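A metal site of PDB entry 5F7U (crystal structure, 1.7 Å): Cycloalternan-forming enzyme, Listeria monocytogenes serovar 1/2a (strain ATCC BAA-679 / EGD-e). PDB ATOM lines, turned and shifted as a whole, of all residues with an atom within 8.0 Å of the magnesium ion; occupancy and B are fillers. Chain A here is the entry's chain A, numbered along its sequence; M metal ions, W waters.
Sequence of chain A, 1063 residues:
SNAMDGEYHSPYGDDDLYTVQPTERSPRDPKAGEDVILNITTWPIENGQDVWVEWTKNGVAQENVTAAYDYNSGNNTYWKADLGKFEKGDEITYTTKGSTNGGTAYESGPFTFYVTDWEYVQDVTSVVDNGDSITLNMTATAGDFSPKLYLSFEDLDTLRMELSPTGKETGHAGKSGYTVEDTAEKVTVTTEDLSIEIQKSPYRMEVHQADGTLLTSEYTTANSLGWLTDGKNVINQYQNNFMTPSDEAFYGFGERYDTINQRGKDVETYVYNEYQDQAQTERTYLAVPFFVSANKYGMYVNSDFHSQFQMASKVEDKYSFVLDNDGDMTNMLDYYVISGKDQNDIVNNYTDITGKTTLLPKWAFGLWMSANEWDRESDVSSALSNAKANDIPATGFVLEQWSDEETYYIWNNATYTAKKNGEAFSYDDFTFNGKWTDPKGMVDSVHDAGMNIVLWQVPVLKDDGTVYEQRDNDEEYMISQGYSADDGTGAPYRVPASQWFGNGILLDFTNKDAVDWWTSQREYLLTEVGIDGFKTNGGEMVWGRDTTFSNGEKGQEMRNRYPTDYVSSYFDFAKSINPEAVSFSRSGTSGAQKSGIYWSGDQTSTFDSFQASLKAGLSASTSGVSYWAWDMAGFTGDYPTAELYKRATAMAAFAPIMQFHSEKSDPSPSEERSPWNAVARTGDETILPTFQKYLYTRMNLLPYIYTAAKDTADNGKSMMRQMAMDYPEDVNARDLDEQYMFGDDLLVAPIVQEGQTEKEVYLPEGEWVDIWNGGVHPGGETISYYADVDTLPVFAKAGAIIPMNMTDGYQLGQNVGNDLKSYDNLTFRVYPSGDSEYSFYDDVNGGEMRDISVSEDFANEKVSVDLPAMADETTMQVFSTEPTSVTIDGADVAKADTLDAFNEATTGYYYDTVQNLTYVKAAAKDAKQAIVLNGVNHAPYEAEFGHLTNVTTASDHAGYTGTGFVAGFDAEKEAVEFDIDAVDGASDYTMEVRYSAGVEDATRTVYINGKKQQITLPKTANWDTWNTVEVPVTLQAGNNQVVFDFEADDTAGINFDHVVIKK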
ATOM      1  N   ALA A 371      -6.985   5.059 -20.384  1.00  0.00           N
ATOM      2  CA  ALA A 371      -8.116   4.161 -20.696  1.00  0.00           C
ATOM      3  C   ALA A 371      -8.924   4.809 -21.792  1.00  0.00           C
ATOM      4  O   ALA A 371      -9.359   5.958 -21.651  1.00  0.00           O
ATOM      5  CB  ALA A 371      -9.011   3.906 -19.471  1.00  0.00           C
ATOM      6  N   ASN A 372      -9.154   4.068 -22.876  1.00  0.00           N
ATOM      7  CA  ASN A 372      -9.925   4.637 -23.976  1.00  0.00           C
ATOM      8  C   ASN A 372     -11.327   5.054 -23.525  1.00  0.00           C
ATOM      9  O   ASN A 372     -11.889   5.996 -24.087  1.00  0.00           O
ATOM     10  CB  ASN A 372     -10.005   3.678 -25.162  1.00  0.00           C
ATOM     11  CG  ASN A 372     -10.582   4.334 -26.393  1.00  0.00           C
ATOM     12  OD1 ASN A 372     -11.774   4.151 -26.708  1.00  0.00           O
ATOM     13  ND2 ASN A 372      -9.764   5.131 -27.078  1.00  0.00           N
ATOM     14  N   GLU A 373     -11.876   4.362 -22.528  1.00  0.00           N
ATOM     15  CA  GLU A 373     -13.232   4.676 -22.036  1.00  0.00           C
ATOM     16  C   GLU A 373     -13.410   6.036 -21.322  1.00  0.00           C
ATOM     17  O   GLU A 373     -14.548   6.485 -21.120  1.00  0.00           O
ATOM     18  CB  GLU A 373     -13.772   3.541 -21.150  1.00  0.00           C
ATOM     19  CG  GLU A 373     -13.075   3.392 -19.805  1.00  0.00           C
ATOM     20  CD  GLU A 373     -13.452   2.091 -19.109  1.00  0.00           C
ATOM     21  OE1 GLU A 373     -13.040   1.003 -19.586  1.00  0.00           O
ATOM     22  OE2 GLU A 373     -14.158   2.171 -18.071  1.00  0.00           O
ATOM     23  N   TRP A 374     -12.302   6.662 -20.934  1.00  0.00           N
ATOM     24  CA  TRP A 374     -12.352   7.988 -20.317  1.00  0.00           C
ATOM     25  C   TRP A 374     -12.699   9.013 -21.383  1.00  0.00           C
ATOM     26  O   TRP A 374     -11.877   9.295 -22.279  1.00  0.00           O
ATOM     27  CB  TRP A 374     -11.023   8.324 -19.644  1.00  0.00           C
ATOM     28  CG  TRP A 374     -10.668   7.412 -18.511  1.00  0.00           C
ATOM     29  CD1 TRP A 374     -11.514   6.573 -17.809  1.00  0.00           C
ATOM     30  CD2 TRP A 374      -9.377   7.260 -17.924  1.00  0.00           C
ATOM     31  NE1 TRP A 374     -10.808   5.893 -16.831  1.00  0.00           N
ATOM     32  CE2 TRP A 374      -9.507   6.319 -16.866  1.00  0.00           C
ATOM     33  CE3 TRP A 374      -8.118   7.826 -18.181  1.00  0.00           C
ATOM     34  CZ2 TRP A 374      -8.409   5.903 -16.093  1.00  0.00           C
ATOM     35  CZ3 TRP A 374      -7.023   7.426 -17.393  1.00  0.00           C
ATOM     36  CH2 TRP A 374      -7.190   6.481 -16.368  1.00  0.00           C
ATOM     37  N   ASP A 375     -13.925   9.526 -21.329  1.00  0.00           N
ATOM     38  CA  ASP A 375     -14.424  10.354 -22.427  1.00  0.00           C
ATOM     39  C   ASP A 375     -15.165  11.589 -21.971  1.00  0.00           C
ATOM     40  O   ASP A 375     -15.883  12.210 -22.766  1.00  0.00           O
ATOM     41  CB  ASP A 375     -15.307   9.526 -23.384  1.00  0.00           C
ATOM     42  CG  ASP A 375     -16.671   9.167 -22.766  1.00  0.00           C
ATOM     43  OD1 ASP A 375     -16.750   8.923 -21.534  1.00  0.00           O
ATOM     44  OD2 ASP A 375     -17.657   9.097 -23.540  1.00  0.00           O
ATOM     45  N   ARG A 376     -15.033  11.933 -20.693  1.00  0.00           N
ATOM     46  CA  ARG A 376     -15.715  13.103 -20.150  1.00  0.00           C
ATOM     47  C   ARG A 376     -15.011  13.561 -18.887  1.00  0.00           C
ATOM     48  O   ARG A 376     -14.240  12.817 -18.297  1.00  0.00           O
ATOM     49  CB  ARG A 376     -17.199  12.804 -19.877  1.00  0.00           C
ATOM     50  CG  ARG A 376     -17.445  11.646 -18.907  1.00  0.00           C
ATOM     51  CD  ARG A 376     -18.885  11.132 -19.067  1.00  0.00           C
ATOM     52  NE  ARG A 376     -18.989  10.242 -20.224  1.00  0.00           N
ATOM     53  CZ  ARG A 376     -20.110   9.992 -20.904  1.00  0.00           C
ATOM     54  NH1 ARG A 376     -21.268  10.566 -20.575  1.00  0.00           N
ATOM     55  NH2 ARG A 376     -20.074   9.159 -21.943  1.00  0.00           N
ATOM     56  N   SER A 378     -16.084  13.929 -15.855  1.00  0.00           N
ATOM     57  CA  SER A 378     -16.332  13.114 -14.656  1.00  0.00           C
ATOM     58  C   SER A 378     -15.494  11.836 -14.654  1.00  0.00           C
ATOM     59  O   SER A 378     -15.163  11.339 -13.588  1.00  0.00           O
ATOM     60  CB  SER A 378     -17.803  12.779 -14.472  1.00  0.00           C
ATOM     61  OG  SER A 378     -18.376  12.176 -15.627  1.00  0.00           O
ATOM     62  N   ASP A 379     -15.143  11.332 -15.841  1.00  0.00           N
ATOM     63  CA  ASP A 379     -14.231  10.170 -15.930  1.00  0.00           C
ATOM     64  C   ASP A 379     -12.834  10.562 -15.454  1.00  0.00           C
ATOM     65  O   ASP A 379     -12.163   9.783 -14.750  1.00  0.00           O
ATOM     66  CB  ASP A 379     -14.111   9.613 -17.375  1.00  0.00           C
ATOM     67  CG  ASP A 379     -15.341   8.785 -17.823  1.00  0.00           C
ATOM     68  OD1 ASP A 379     -16.174   8.406 -16.979  1.00  0.00           O
ATOM     69  OD2 ASP A 379     -15.469   8.491 -19.035  1.00  0.00           O
ATOM     70  N   VAL A 380     -12.390  11.750 -15.857  1.00  0.00           N
ATOM     71  CA  VAL A 380     -11.063  12.242 -15.460  1.00  0.00           C
ATOM     72  C   VAL A 380     -11.062  12.488 -13.935  1.00  0.00           C
ATOM     73  O   VAL A 380     -10.134  12.033 -13.257  1.00  0.00           O
ATOM     74  CB  VAL A 380     -10.650  13.516 -16.245  1.00  0.00           C
ATOM     75  CG1 VAL A 380      -9.363  14.123 -15.676  1.00  0.00           C
ATOM     76  CG2 VAL A 380     -10.440  13.182 -17.712  1.00  0.00           C
ATOM     77  N   GLN A 401     -10.230   9.508 -25.946  1.00  0.00           N
ATOM     78  CA  GLN A 401     -11.584   9.803 -26.381  1.00  0.00           C
ATOM     79  C   GLN A 401     -11.993  11.227 -25.926  1.00  0.00           C
ATOM     80  O   GLN A 401     -12.963  11.432 -25.183  1.00  0.00           O
ATOM     81  CB  GLN A 401     -12.536   8.708 -25.867  1.00  0.00           C
ATOM     82  CG  GLN A 401     -13.804   8.609 -26.689  1.00  0.00           C
ATOM     83  CD  GLN A 401     -14.765   7.514 -26.253  1.00  0.00           C
ATOM     84  OE1 GLN A 401     -15.901   7.517 -26.723  1.00  0.00           O
ATOM     85  NE2 GLN A 401     -14.354   6.622 -25.352  1.00  0.00           N
ATOM     86  N   LYS A 435     -19.717  16.894 -22.310  1.00  0.00           N
ATOM     87  CA  LYS A 435     -18.687  16.057 -21.708  1.00  0.00           C
ATOM     88  C   LYS A 435     -17.454  16.823 -21.229  1.00  0.00           C
ATOM     89  O   LYS A 435     -16.730  16.350 -20.327  1.00  0.00           O
ATOM     90  CB  LYS A 435     -18.289  14.932 -22.671  1.00  0.00           C
ATOM     91  CG  LYS A 435     -19.442  13.955 -22.902  1.00  0.00           C
ATOM     92  CD  LYS A 435     -19.172  13.004 -24.058  1.00  0.00           C
ATOM     93  CE  LYS A 435     -20.389  12.125 -24.276  1.00  0.00           C
ATOM     94  NZ  LYS A 435     -20.350  11.437 -25.597  1.00  0.00           N
ATOM     95  N   LYS A 664     -11.382  -0.632 -24.886  1.00  0.00           N
ATOM     96  CA  LYS A 664     -12.829  -0.469 -25.148  1.00  0.00           C
ATOM     97  C   LYS A 664     -13.326   0.945 -24.849  1.00  0.00           C
ATOM     98  O   LYS A 664     -12.904   1.583 -23.880  1.00  0.00           O
ATOM     99  CB  LYS A 664     -13.664  -1.520 -24.399  1.00  0.00           C
ATOM    100  CG  LYS A 664     -13.384  -2.980 -24.801  1.00  0.00           C
ATOM    101  CD  LYS A 664     -13.665  -3.246 -26.275  1.00  0.00           C
ATOM    102  CE  LYS A 664     -13.591  -4.727 -26.588  1.00  0.00           C
ATOM    103  NZ  LYS A 664     -12.781  -5.003 -27.808  1.00  0.00           N
ATOM    104  N   SER A 665     -14.226   1.433 -25.701  1.00  0.00           N
ATOM    105  CA  SER A 665     -14.622   2.845 -25.624  1.00  0.00           C
ATOM    106  C   SER A 665     -15.766   3.123 -24.651  1.00  0.00           C
ATOM    107  O   SER A 665     -15.835   4.221 -24.109  1.00  0.00           O
ATOM    108  CB  SER A 665     -14.978   3.372 -27.022  1.00  0.00           C
ATOM    109  OG  SER A 665     -16.099   2.659 -27.535  1.00  0.00           O
ATOM    110  N   ASP A 666     -16.665   2.160 -24.449  1.00  0.00           N
ATOM    111  CA  ASP A 666     -17.803   2.362 -23.521  1.00  0.00           C
ATOM    112  C   ASP A 666     -18.267   1.016 -22.939  1.00  0.00           C
ATOM    113  O   ASP A 666     -19.416   0.613 -23.129  1.00  0.00           O
ATOM    114  CB  ASP A 666     -18.946   3.097 -24.237  1.00  0.00           C
ATOM    115  CG  ASP A 666     -20.058   3.535 -23.297  1.00  0.00           C
ATOM    116  OD1 ASP A 666     -19.832   3.729 -22.071  1.00  0.00           O
ATOM    117  OD2 ASP A 666     -21.191   3.694 -23.802  1.00  0.00           O
ATOM    118  N   PRO A 667     -17.365   0.319 -22.235  1.00  0.00           N
ATOM    119  CA  PRO A 667     -17.713  -1.021 -21.780  1.00  0.00           C
ATOM    120  C   PRO A 667     -18.491  -1.000 -20.474  1.00  0.00           C
ATOM    121  O   PRO A 667     -18.434  -0.019 -19.732  1.00  0.00           O
ATOM    122  CB  PRO A 667     -16.329  -1.658 -21.559  1.00  0.00           C
ATOM    123  CG  PRO A 667     -15.494  -0.518 -21.084  1.00  0.00           C
ATOM    124  CD  PRO A 667     -15.965   0.671 -21.889  1.00  0.00           C
HETATM  125 MG    MG M   1     -16.526   7.086 -20.355  1.00  0.00          MG
HETATM  126  O   HOH W   1     -16.229   5.534 -18.659  1.00  0.00           O
HETATM  127  O   HOH W   2     -17.234   5.859 -22.193  1.00  0.00           O
HETATM  128  O   HOH W   3     -18.416   7.498 -19.343  1.00  0.00           O
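The guanidinium group (NH2) of Arg 376 lies within salt-bridge range of the side-chain carboxylate (OD2) of Asp 375 (2.9 Å).
The backbone NH of Glu 373 sits at hydrogen-bond distance from the backbone carbonyl oxygen of Lys 664, at 3.3 Å.
The magnesium ion is bound by water W3, the side-chain carboxylate of Asp 375, the side-chain carboxylate of Asp 379, the backbone carbonyl oxygen of Glu 373, water W1 and water W2.
The magnesium ion has six donor atoms within binding distance.
Water W3 lies within hydrogen-bond range of NE of Arg 376 (2.9 Å) and OD1 of Asp 379 (3.4 Å).
Water W2 lies within hydrogen-bond range of the backbone carbonyl oxygen (O) of Ser 665 (2.9 Å) and the side-chain carboxylate (OD1) of Asp 666 (3.4 Å).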
